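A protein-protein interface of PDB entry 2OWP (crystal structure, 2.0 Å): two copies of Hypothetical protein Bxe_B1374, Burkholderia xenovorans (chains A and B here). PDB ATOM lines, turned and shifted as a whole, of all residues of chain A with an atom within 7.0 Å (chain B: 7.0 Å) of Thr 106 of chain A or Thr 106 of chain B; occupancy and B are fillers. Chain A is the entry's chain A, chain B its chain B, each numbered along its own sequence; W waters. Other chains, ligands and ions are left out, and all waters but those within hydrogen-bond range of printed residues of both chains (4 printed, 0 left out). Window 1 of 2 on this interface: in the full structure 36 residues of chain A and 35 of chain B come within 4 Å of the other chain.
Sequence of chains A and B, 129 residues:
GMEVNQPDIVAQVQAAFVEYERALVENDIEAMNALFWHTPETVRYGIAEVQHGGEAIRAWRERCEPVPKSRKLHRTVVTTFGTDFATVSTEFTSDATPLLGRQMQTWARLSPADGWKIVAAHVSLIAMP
Phe 81 of chain A touches Phe 85 of chain B, and with the chains exchanged Phe 85 of chain A touches Phe 81 of chain B.
Phe 85 of chain A touches its own counterpart, Phe 85 of chain B.
Phe 85 of chain A touches Thr 106 of chain B, but with the chains exchanged Thr 106 of chain A does not touch Phe 85 of chain B (6.9 Å).
Thr 87 of chain A touches Thr 106 of chain B, and with the chains exchanged Thr 106 of chain A touches Thr 87 of chain B.
16 positions are printed for both chains.
A ring nitrogen (ND1) of His 122 of chain B lies within hydrogen-bond range of the backbone carbonyl oxygen (O) of His 122 of chain A.
The backbone NH (N) of Ala 121 of chain A sits close to the side-chain sulfur (SD) of Met 104 of chain B, 3.6 Å away.
The side-chain hydroxyl (OG1) of Thr 106 of chain A lies within hydrogen-bond range of the side-chain hydroxyl (OG1) of Thr 106 of chain B.
The side-chain sulfur of Met 104 of chain A lies close to the backbone NH of Ala 121 of chain B.
Printed residues of chain A that touch a printed residue of chain B: Phe 81, Phe 85, Thr 87, Met 104, Thr 106, Val 119, Ala 120, Ala 121 and His 122.
Of the 16 printed residues of chain B, 9 touch a printed residue of chain A.
Printed residues of chain B that touch a printed residue of chain A: Phe 81, Phe 85, Thr 87, Met 104, Thr 106, Val 119, Ala 120, Ala 121 and His 122.
Among the printed residues, no Asp or Glu carboxylate lies within 4 Å of a Lys or Arg side-chain nitrogen of the other chain.
Ile 118 of chain A touches none of the printed residues of chain B.
Printed residues of chain B within 4 Å of Ala 120 of chain A: Met 104 (3.7 Å).
Printed residues of chain A within 4 Å of Thr 87 of chain B: Thr 106 (3.7 Å).
Thr 106 of chain B touches just these residues of chain A: Phe 85, Thr 87 and Thr 106.
Of the printed residues of chain A, Val 119 of chain B touches Phe 81.
Of the printed residues of chain A, Ala 121 of chain B touches Met 104.
The nearest printed residue of chain B that does not touch Ala 120 of chain A is Thr 87 of chain B (4.1 Å).
Among the printed residues, pairs that only touch across the chains: Phe 81 of chain A with Phe 85 of chain B (3.7 Å), Phe 81 of chain A with Val 119 of chain B (3.8 Å), Phe 85 of chain A with Phe 81 of chain B (3.97 Å), Phe 85 of chain A with Phe 85 of chain B (3.3 Å), Phe 85 of chain A with Thr 106 of chain B (3.5 Å), Thr 87 of chain A with Thr 106 of chain B (3.6 Å), Thr 87 of chain A with Ala 120 of chain B (3.9 Å), Met 104 of chain A with Ala 120 of chain B (3.8 Å), Met 104 of chain A with His 122 of chain B (3.8 Å), Thr 106 of chain A with Thr 87 of chain B (3.7 Å), Val 119 of chain A with Phe 81 of chain B (3.8 Å), Ala 120 of chain A with Met 104 of chain B (3.7 Å) and His 122 of chain A with Met 104 of chain B (3.8 Å).
Water W3 bridges the side-chain hydroxyl of Thr 87 of chain A and the backbone carbonyl oxygen of Val 119 of chain B.
Water W4 lies within hydrogen-bond range of the side-chain hydroxyl (OG1) of Thr 106 of chain B, the side-chain sulfur (SD) of Met 104 of chain A and the backbone carbonyl oxygen (O) of Met 104 of chain B.
Water W2 lies within hydrogen-bond range of the side-chain hydroxyl (OG1) of Thr 106 of chain A, the backbone carbonyl oxygen (O) of Met 104 of chain A and the side-chain sulfur (SD) of Met 104 of chain B.
Water W1 bridges the backbone carbonyl oxygen (O) of Val 119 of chain A (2.9 Å) and the side-chain hydroxyl (OG1) of Thr 87 of chain B (2.9 Å).
The backbone carbonyl oxygen (O) of Thr 106 of chain B sits at hydrogen-bond distance from the backbone NH (N) of Val 119 of chain B (2.8 Å).
O of Thr 106 of chain A lies within hydrogen-bond range of N of Val 119 of chain A (2.8 Å).
The backbone carbonyl oxygen (O) of His 122 of chain B lies within hydrogen-bond range of the backbone NH (N) of Met 104 of chain B.
The backbone carbonyl oxygen (O) of His 122 of chain A sits at hydrogen-bond distance from the backbone NH (N) of Met 104 of chain A.
O of Ala 120 of chain A is in hydrogen-bond range of N of Thr 106 of chain A (2.9 Å).
N of Thr 106 of chain B is in hydrogen-bond range of O of Ala 120 of chain B (2.9 Å).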
ATOM      1  N   PHE A  81     -22.326   3.192   7.774  1.00  0.00           N
ATOM      2  CA  PHE A  81     -23.065   3.338   6.528  1.00  0.00           C
ATOM      3  C   PHE A  81     -23.144   1.956   5.898  1.00  0.00           C
ATOM      4  O   PHE A  81     -22.121   1.384   5.548  1.00  0.00           O
ATOM      5  CB  PHE A  81     -22.372   4.327   5.599  1.00  0.00           C
ATOM      6  CG  PHE A  81     -22.043   5.661   6.264  1.00  0.00           C
ATOM      7  CD1 PHE A  81     -20.855   5.830   6.942  1.00  0.00           C
ATOM      8  CD2 PHE A  81     -22.946   6.709   6.214  1.00  0.00           C
ATOM      9  CE1 PHE A  81     -20.563   6.991   7.580  1.00  0.00           C
ATOM     10  CE2 PHE A  81     -22.652   7.913   6.829  1.00  0.00           C
ATOM     11  CZ  PHE A  81     -21.434   8.047   7.512  1.00  0.00           C
ATOM     12  N   PHE A  85     -18.896   0.156   6.219  1.00  0.00           N
ATOM     13  CA  PHE A  85     -18.177   1.430   6.271  1.00  0.00           C
ATOM     14  C   PHE A  85     -18.584   2.228   7.468  1.00  0.00           C
ATOM     15  O   PHE A  85     -19.727   2.155   7.898  1.00  0.00           O
ATOM     16  CB  PHE A  85     -18.495   2.238   5.024  1.00  0.00           C
ATOM     17  CG  PHE A  85     -17.455   3.241   4.661  1.00  0.00           C
ATOM     18  CD1 PHE A  85     -16.183   2.833   4.258  1.00  0.00           C
ATOM     19  CD2 PHE A  85     -17.767   4.602   4.624  1.00  0.00           C
ATOM     20  CE1 PHE A  85     -15.231   3.773   3.874  1.00  0.00           C
ATOM     21  CE2 PHE A  85     -16.849   5.512   4.234  1.00  0.00           C
ATOM     22  CZ  PHE A  85     -15.565   5.096   3.855  1.00  0.00           C
ATOM     23  N   ALA A  86     -17.648   3.042   7.997  1.00  0.00           N
ATOM     24  CA  ALA A  86     -17.928   3.814   9.190  1.00  0.00           C
ATOM     25  C   ALA A  86     -16.908   4.919   9.372  1.00  0.00           C
ATOM     26  O   ALA A  86     -15.804   4.873   8.839  1.00  0.00           O
ATOM     27  CB  ALA A  86     -17.923   2.907  10.430  1.00  0.00           C
ATOM     28  N   THR A  87     -17.306   5.908  10.146  1.00  0.00           N
ATOM     29  CA  THR A  87     -16.398   6.934  10.661  1.00  0.00           C
ATOM     30  C   THR A  87     -16.527   6.918  12.184  1.00  0.00           C
ATOM     31  O   THR A  87     -17.626   6.709  12.721  1.00  0.00           O
ATOM     32  CB  THR A  87     -16.714   8.396  10.135  1.00  0.00           C
ATOM     33  OG1 THR A  87     -18.030   8.809  10.512  1.00  0.00           O
ATOM     34  CG2 THR A  87     -16.587   8.510   8.612  1.00  0.00           C
ATOM     35  N   VAL A  88     -15.396   7.049  12.849  1.00  0.00           N
ATOM     36  CA  VAL A  88     -15.350   7.266  14.295  1.00  0.00           C
ATOM     37  C   VAL A  88     -14.544   8.516  14.556  1.00  0.00           C
ATOM     38  O   VAL A  88     -13.363   8.587  14.192  1.00  0.00           O
ATOM     39  CB  VAL A  88     -14.720   6.084  15.098  1.00  0.00           C
ATOM     40  CG1 VAL A  88     -14.886   6.339  16.602  1.00  0.00           C
ATOM     41  CG2 VAL A  88     -15.401   4.744  14.754  1.00  0.00           C
ATOM     42  N   MET A 104     -10.050  11.452  13.911  1.00  0.00           N
ATOM     43  CA  MET A 104     -11.077  10.958  13.032  1.00  0.00           C
ATOM     44  C   MET A 104     -10.516   9.800  12.240  1.00  0.00           C
ATOM     45  O   MET A 104      -9.500   9.946  11.577  1.00  0.00           O
ATOM     46  CB  MET A 104     -11.538  12.027  12.059  1.00  0.00           C
ATOM     47  CG  MET A 104     -12.740  11.658  11.259  1.00  0.00           C
ATOM     48  SD  MET A 104     -13.290  13.216  10.261  1.00  0.00           S
ATOM     49  CE  MET A 104     -14.275  14.241  11.678  1.00  0.00           C
ATOM     50  N   GLN A 105     -11.197   8.666  12.333  1.00  0.00           N
ATOM     51  CA  GLN A 105     -10.808   7.437  11.648  1.00  0.00           C
ATOM     52  C   GLN A 105     -11.910   6.998  10.730  1.00  0.00           C
ATOM     53  O   GLN A 105     -13.087   7.028  11.119  1.00  0.00           O
ATOM     54  CB  GLN A 105     -10.581   6.327  12.647  1.00  0.00           C
ATOM     55  CG  GLN A 105      -9.479   6.594  13.702  1.00  0.00           C
ATOM     56  CD  GLN A 105      -9.564   5.614  14.860  1.00  0.00           C
ATOM     57  OE1 GLN A 105     -10.651   5.158  15.206  1.00  0.00           O
ATOM     58  NE2 GLN A 105      -8.415   5.229  15.398  1.00  0.00           N
ATOM     59  N   THR A 106     -11.542   6.605   9.504  1.00  0.00           N
ATOM     60  CA  THR A 106     -12.473   6.000   8.575  1.00  0.00           C
ATOM     61  C   THR A 106     -12.193   4.513   8.634  1.00  0.00           C
ATOM     62  O   THR A 106     -11.041   4.081   8.469  1.00  0.00           O
ATOM     63  CB  THR A 106     -12.251   6.532   7.139  1.00  0.00           C
ATOM     64  OG1 THR A 106     -12.330   7.965   7.188  1.00  0.00           O
ATOM     65  CG2 THR A 106     -13.280   5.999   6.210  1.00  0.00           C
ATOM     66  N   TRP A 107     -13.256   3.742   8.869  1.00  0.00           N
ATOM     67  CA  TRP A 107     -13.197   2.303   9.020  1.00  0.00           C
ATOM     68  C   TRP A 107     -13.954   1.660   7.885  1.00  0.00           C
ATOM     69  O   TRP A 107     -15.029   2.143   7.478  1.00  0.00           O
ATOM     70  CB  TRP A 107     -13.854   1.856  10.335  1.00  0.00           C
ATOM     71  CG  TRP A 107     -13.130   2.188  11.590  1.00  0.00           C
ATOM     72  CD1 TRP A 107     -13.074   3.411  12.223  1.00  0.00           C
ATOM     73  CD2 TRP A 107     -12.369   1.281  12.401  1.00  0.00           C
ATOM     74  NE1 TRP A 107     -12.315   3.319  13.374  1.00  0.00           N
ATOM     75  CE2 TRP A 107     -11.854   2.027  13.500  1.00  0.00           C
ATOM     76  CE3 TRP A 107     -12.041  -0.084  12.292  1.00  0.00           C
ATOM     77  CZ2 TRP A 107     -11.034   1.446  14.492  1.00  0.00           C
ATOM     78  CZ3 TRP A 107     -11.243  -0.661  13.280  1.00  0.00           C
ATOM     79  CH2 TRP A 107     -10.742   0.105  14.364  1.00  0.00           C
ATOM     80  N   ALA A 108     -13.429   0.530   7.416  1.00  0.00           N
ATOM     81  CA  ALA A 108     -14.079  -0.250   6.377  1.00  0.00           C
ATOM     82  C   ALA A 108     -13.815  -1.717   6.649  1.00  0.00           C
ATOM     83  O   ALA A 108     -12.788  -2.073   7.249  1.00  0.00           O
ATOM     84  CB  ALA A 108     -13.533   0.134   4.978  1.00  0.00           C
ATOM     85  N   LYS A 117     -11.157  -2.569   9.598  1.00  0.00           N
ATOM     86  CA  LYS A 117      -9.862  -1.910   9.668  1.00  0.00           C
ATOM     87  C   LYS A 117      -9.981  -0.425   9.466  1.00  0.00           C
ATOM     88  O   LYS A 117     -10.930   0.056   8.844  1.00  0.00           O
ATOM     89  CB  LYS A 117      -8.902  -2.495   8.625  1.00  0.00           C
ATOM     90  CG  LYS A 117      -8.579  -3.976   8.862  1.00  0.00           C
ATOM     91  CD  LYS A 117      -7.411  -4.394   8.023  1.00  0.00           C
ATOM     92  CE  LYS A 117      -7.209  -5.910   7.985  1.00  0.00           C
ATOM     93  NZ  LYS A 117      -6.183  -6.315   8.974  1.00  0.00           N
ATOM     94  N   ILE A 118      -9.010   0.303   9.992  1.00  0.00           N
ATOM     95  CA  ILE A 118      -8.895   1.759   9.745  1.00  0.00           C
ATOM     96  C   ILE A 118      -8.160   1.951   8.409  1.00  0.00           C
ATOM     97  O   ILE A 118      -7.000   1.515   8.232  1.00  0.00           O
ATOM     98  CB  ILE A 118      -8.114   2.496  10.868  1.00  0.00           C
ATOM     99  CG1 ILE A 118      -8.738   2.233  12.235  1.00  0.00           C
ATOM    100  CG2 ILE A 118      -8.058   4.000  10.598  1.00  0.00           C
ATOM    101  CD1 ILE A 118      -7.825   2.543  13.439  1.00  0.00           C
ATOM    102  N   VAL A 119      -8.824   2.603   7.474  1.00  0.00           N
ATOM    103  CA  VAL A 119      -8.255   2.845   6.154  1.00  0.00           C
ATOM    104  C   VAL A 119      -7.650   4.244   6.005  1.00  0.00           C
ATOM    105  O   VAL A 119      -6.900   4.474   5.067  1.00  0.00           O
ATOM    106  CB  VAL A 119      -9.312   2.637   5.044  1.00  0.00           C
ATOM    107  CG1 VAL A 119      -9.714   1.131   4.946  1.00  0.00           C
ATOM    108  CG2 VAL A 119     -10.493   3.510   5.302  1.00  0.00           C
ATOM    109  N   ALA A 120      -8.025   5.170   6.892  1.00  0.00           N
ATOM    110  CA  ALA A 120      -7.431   6.493   6.943  1.00  0.00           C
ATOM    111  C   ALA A 120      -7.650   7.069   8.331  1.00  0.00           C
ATOM    112  O   ALA A 120      -8.681   6.828   8.943  1.00  0.00           O
ATOM    113  CB  ALA A 120      -8.064   7.404   5.877  1.00  0.00           C
ATOM    114  N   ALA A 121      -6.676   7.827   8.847  1.00  0.00           N
ATOM    115  CA  ALA A 121      -6.872   8.519  10.111  1.00  0.00           C
ATOM    116  C   ALA A 121      -6.186   9.862  10.126  1.00  0.00           C
ATOM    117  O   ALA A 121      -5.170  10.019   9.498  1.00  0.00           O
ATOM    118  CB  ALA A 121      -6.423   7.678  11.259  1.00  0.00           C
ATOM    119  N   HIS A 122      -6.806  10.815  10.829  1.00  0.00           N
ATOM    120  CA  HIS A 122      -6.272  12.159  11.034  1.00  0.00           C
ATOM    121  C   HIS A 122      -6.413  12.504  12.518  1.00  0.00           C
ATOM    122  O   HIS A 122      -7.522  12.432  13.071  1.00  0.00           O
ATOM    123  CB  HIS A 122      -7.119  13.126  10.218  1.00  0.00           C
ATOM    124  CG  HIS A 122      -6.590  14.513  10.139  1.00  0.00           C
ATOM    125  ND1 HIS A 122      -7.070  15.409   9.222  1.00  0.00           N
ATOM    126  CD2 HIS A 122      -5.643  15.174  10.852  1.00  0.00           C
ATOM    127  CE1 HIS A 122      -6.436  16.562   9.357  1.00  0.00           C
ATOM    128  NE2 HIS A 122      -5.570  16.450  10.348  1.00  0.00           N
ATOM    129  N   PHE B  81     -13.784   2.770  -2.111  1.00  0.00           N
ATOM    130  CA  PHE B  81     -14.058   1.402  -1.703  1.00  0.00           C
ATOM    131  C   PHE B  81     -15.413   1.044  -2.263  1.00  0.00           C
ATOM    132  O   PHE B  81     -16.403   1.718  -1.965  1.00  0.00           O
ATOM    133  CB  PHE B  81     -14.042   1.294  -0.183  1.00  0.00           C
ATOM    134  CG  PHE B  81     -12.808   1.903   0.440  1.00  0.00           C
ATOM    135  CD1 PHE B  81     -11.659   1.158   0.622  1.00  0.00           C
ATOM    136  CD2 PHE B  81     -12.794   3.218   0.792  1.00  0.00           C
ATOM    137  CE1 PHE B  81     -10.533   1.730   1.203  1.00  0.00           C
ATOM    138  CE2 PHE B  81     -11.668   3.801   1.340  1.00  0.00           C
ATOM    139  CZ  PHE B  81     -10.534   3.065   1.520  1.00  0.00           C
ATOM    140  N   PHE B  85     -18.188   4.615  -1.382  1.00  0.00           N
ATOM    141  CA  PHE B  85     -17.436   5.159  -0.251  1.00  0.00           C
ATOM    142  C   PHE B  85     -16.065   5.575  -0.696  1.00  0.00           C
ATOM    143  O   PHE B  85     -15.499   4.969  -1.606  1.00  0.00           O
ATOM    144  CB  PHE B  85     -17.206   4.091   0.819  1.00  0.00           C
ATOM    145  CG  PHE B  85     -18.421   3.399   1.270  1.00  0.00           C
ATOM    146  CD1 PHE B  85     -19.474   4.120   1.843  1.00  0.00           C
ATOM    147  CD2 PHE B  85     -18.498   1.993   1.217  1.00  0.00           C
ATOM    148  CE1 PHE B  85     -20.593   3.468   2.314  1.00  0.00           C
ATOM    149  CE2 PHE B  85     -19.619   1.315   1.698  1.00  0.00           C
ATOM    150  CZ  PHE B  85     -20.682   2.040   2.227  1.00  0.00           C
ATOM    151  N   ALA B  86     -15.508   6.571  -0.034  1.00  0.00           N
ATOM    152  CA  ALA B  86     -14.189   7.067  -0.381  1.00  0.00           C
ATOM    153  C   ALA B  86     -13.601   7.893   0.755  1.00  0.00           C
ATOM    154  O   ALA B  86     -14.337   8.422   1.627  1.00  0.00           O
ATOM    155  CB  ALA B  86     -14.228   7.939  -1.698  1.00  0.00           C
ATOM    156  N   THR B  87     -12.283   8.028   0.715  1.00  0.00           N
ATOM    157  CA  THR B  87     -11.616   9.071   1.471  1.00  0.00           C
ATOM    158  C   THR B  87     -10.800   9.927   0.531  1.00  0.00           C
ATOM    159  O   THR B  87     -10.202   9.412  -0.411  1.00  0.00           O
ATOM    160  CB  THR B  87     -10.657   8.490   2.522  1.00  0.00           C
ATOM    161  OG1 THR B  87      -9.653   7.708   1.877  1.00  0.00           O
ATOM    162  CG2 THR B  87     -11.402   7.641   3.530  1.00  0.00           C
ATOM    163  N   VAL B  88     -10.750  11.227   0.802  1.00  0.00           N
ATOM    164  CA  VAL B  88      -9.813  12.104   0.128  1.00  0.00           C
ATOM    165  C   VAL B  88      -8.975  12.829   1.149  1.00  0.00           C
ATOM    166  O   VAL B  88      -9.489  13.561   2.005  1.00  0.00           O
ATOM    167  CB  VAL B  88     -10.561  13.121  -0.772  1.00  0.00           C
ATOM    168  CG1 VAL B  88      -9.573  13.987  -1.582  1.00  0.00           C
ATOM    169  CG2 VAL B  88     -11.490  12.417  -1.702  1.00  0.00           C
ATOM    170  N   MET B 104      -8.653  15.803   5.697  1.00  0.00           N
ATOM    171  CA  MET B 104      -9.115  14.451   5.326  1.00  0.00           C
ATOM    172  C   MET B 104     -10.581  14.463   5.364  1.00  0.00           C
ATOM    173  O   MET B 104     -11.133  14.824   6.387  1.00  0.00           O
ATOM    174  CB  MET B 104      -8.609  13.381   6.295  1.00  0.00           C
ATOM    175  CG  MET B 104      -8.938  11.950   5.938  1.00  0.00           C
ATOM    176  SD  MET B 104      -7.978  10.810   7.212  1.00  0.00           S
ATOM    177  CE  MET B 104      -6.137  10.932   6.475  1.00  0.00           C
ATOM    178  N   GLN B 105     -11.201  13.986   4.276  1.00  0.00           N
ATOM    179  CA  GLN B 105     -12.651  13.959   4.104  1.00  0.00           C
ATOM    180  C   GLN B 105     -13.105  12.550   3.855  1.00  0.00           C
ATOM    181  O   GLN B 105     -12.470  11.846   3.083  1.00  0.00           O
ATOM    182  CB  GLN B 105     -13.036  14.775   2.888  1.00  0.00           C
ATOM    183  CG  GLN B 105     -12.792  16.262   3.042  1.00  0.00           C
ATOM    184  CD  GLN B 105     -12.968  17.019   1.735  1.00  0.00           C
ATOM    185  OE1 GLN B 105     -12.839  16.470   0.660  1.00  0.00           O
ATOM    186  NE2 GLN B 105     -13.234  18.282   1.840  1.00  0.00           N
ATOM    187  N   THR B 106     -14.174  12.126   4.515  1.00  0.00           N
ATOM    188  CA  THR B 106     -14.763  10.825   4.199  1.00  0.00           C
ATOM    189  C   THR B 106     -15.987  11.163   3.367  1.00  0.00           C
ATOM    190  O   THR B 106     -16.811  12.000   3.769  1.00  0.00           O
ATOM    191  CB  THR B 106     -15.174  10.073   5.461  1.00  0.00           C
ATOM    192  OG1 THR B 106     -14.065   9.956   6.340  1.00  0.00           O
ATOM    193  CG2 THR B 106     -15.763   8.682   5.149  1.00  0.00           C
ATOM    194  N   TRP B 107     -16.111  10.471   2.232  1.00  0.00           N
ATOM    195  CA  TRP B 107     -17.172  10.677   1.257  1.00  0.00           C
ATOM    196  C   TRP B 107     -18.012   9.422   1.106  1.00  0.00           C
ATOM    197  O   TRP B 107     -17.484   8.305   1.142  1.00  0.00           O
ATOM    198  CB  TRP B 107     -16.524  10.965  -0.088  1.00  0.00           C
ATOM    199  CG  TRP B 107     -15.871  12.323  -0.237  1.00  0.00           C
ATOM    200  CD1 TRP B 107     -14.620  12.718   0.182  1.00  0.00           C
ATOM    201  CD2 TRP B 107     -16.437  13.433  -0.920  1.00  0.00           C
ATOM    202  NE1 TRP B 107     -14.398  13.999  -0.188  1.00  0.00           N
ATOM    203  CE2 TRP B 107     -15.501  14.472  -0.865  1.00  0.00           C
ATOM    204  CE3 TRP B 107     -17.687  13.664  -1.534  1.00  0.00           C
ATOM    205  CZ2 TRP B 107     -15.745  15.727  -1.425  1.00  0.00           C
ATOM    206  CZ3 TRP B 107     -17.932  14.915  -2.075  1.00  0.00           C
ATOM    207  CH2 TRP B 107     -16.948  15.935  -2.016  1.00  0.00           C
ATOM    208  N   ALA B 108     -19.310   9.611   0.920  1.00  0.00           N
ATOM    209  CA  ALA B 108     -20.237   8.541   0.725  1.00  0.00           C
ATOM    210  C   ALA B 108     -21.314   8.973  -0.249  1.00  0.00           C
ATOM    211  O   ALA B 108     -21.696  10.142  -0.297  1.00  0.00           O
ATOM    212  CB  ALA B 108     -20.873   8.104   2.070  1.00  0.00           C
ATOM    213  N   LYS B 117     -21.398  12.894  -1.119  1.00  0.00           N
ATOM    214  CA  LYS B 117     -21.318  13.908  -0.062  1.00  0.00           C
ATOM    215  C   LYS B 117     -20.192  13.581   0.916  1.00  0.00           C
ATOM    216  O   LYS B 117     -19.820  12.419   1.077  1.00  0.00           O
ATOM    217  CB  LYS B 117     -22.652  14.010   0.689  1.00  0.00           C
ATOM    218  CG  LYS B 117     -23.713  14.879  -0.040  1.00  0.00           C
ATOM    219  CD  LYS B 117     -25.089  14.552   0.477  1.00  0.00           C
ATOM    220  CE  LYS B 117     -26.213  15.418  -0.142  1.00  0.00           C
ATOM    221  NZ  LYS B 117     -25.928  15.856  -1.505  1.00  0.00           N
ATOM    222  N   ILE B 118     -19.659  14.629   1.545  1.00  0.00           N
ATOM    223  CA  ILE B 118     -18.718  14.541   2.641  1.00  0.00           C
ATOM    224  C   ILE B 118     -19.501  14.251   3.891  1.00  0.00           C
ATOM    225  O   ILE B 118     -20.374  15.022   4.261  1.00  0.00           O
ATOM    226  CB  ILE B 118     -17.942  15.885   2.856  1.00  0.00           C
ATOM    227  CG1 ILE B 118     -17.133  16.261   1.621  1.00  0.00           C
ATOM    228  CG2 ILE B 118     -17.015  15.786   4.059  1.00  0.00           C
ATOM    229  CD1 ILE B 118     -16.954  17.737   1.432  1.00  0.00           C
ATOM    230  N   VAL B 119     -19.243  13.108   4.528  1.00  0.00           N
ATOM    231  CA  VAL B 119     -19.967  12.764   5.746  1.00  0.00           C
ATOM    232  C   VAL B 119     -19.178  13.073   7.013  1.00  0.00           C
ATOM    233  O   VAL B 119     -19.750  13.062   8.113  1.00  0.00           O
ATOM    234  CB  VAL B 119     -20.364  11.284   5.791  1.00  0.00           C
ATOM    235  CG1 VAL B 119     -21.358  10.990   4.671  1.00  0.00           C
ATOM    236  CG2 VAL B 119     -19.128  10.389   5.706  1.00  0.00           C
ATOM    237  N   ALA B 120     -17.876  13.299   6.860  1.00  0.00           N
ATOM    238  CA  ALA B 120     -17.042  13.672   7.990  1.00  0.00           C
ATOM    239  C   ALA B 120     -15.783  14.363   7.467  1.00  0.00           C
ATOM    240  O   ALA B 120     -15.299  13.984   6.422  1.00  0.00           O
ATOM    241  CB  ALA B 120     -16.688  12.386   8.825  1.00  0.00           C
ATOM    242  N   ALA B 121     -15.287  15.406   8.141  1.00  0.00           N
ATOM    243  CA  ALA B 121     -14.015  16.046   7.703  1.00  0.00           C
ATOM    244  C   ALA B 121     -13.171  16.491   8.875  1.00  0.00           C
ATOM    245  O   ALA B 121     -13.683  16.853   9.928  1.00  0.00           O
ATOM    246  CB  ALA B 121     -14.273  17.244   6.747  1.00  0.00           C
ATOM    247  N   HIS B 122     -11.854  16.418   8.703  1.00  0.00           N
ATOM    248  CA  HIS B 122     -10.914  16.874   9.738  1.00  0.00           C
ATOM    249  C   HIS B 122      -9.826  17.694   9.054  1.00  0.00           C
ATOM    250  O   HIS B 122      -9.214  17.244   8.108  1.00  0.00           O
ATOM    251  CB  HIS B 122     -10.348  15.658  10.448  1.00  0.00           C
ATOM    252  CG  HIS B 122      -9.448  15.956  11.619  1.00  0.00           C
ATOM    253  ND1 HIS B 122      -9.026  14.969  12.473  1.00  0.00           N
ATOM    254  CD2 HIS B 122      -8.946  17.117  12.114  1.00  0.00           C
ATOM    255  CE1 HIS B 122      -8.246  15.491  13.404  1.00  0.00           C
ATOM    256  NE2 HIS B 122      -8.201  16.795  13.221  1.00  0.00           N
HETATM  257  O   HOH W   1      -8.093   5.349   2.626  1.00  0.00           O
HETATM  258  O   HOH W   2     -10.942   9.835   8.616  1.00  0.00           O
HETATM  259  O   HOH W   3     -19.838  10.536   9.655  1.00  0.00           O
HETATM  260  O   HOH W   4     -12.392  11.840   7.319  1.00  0.00           O
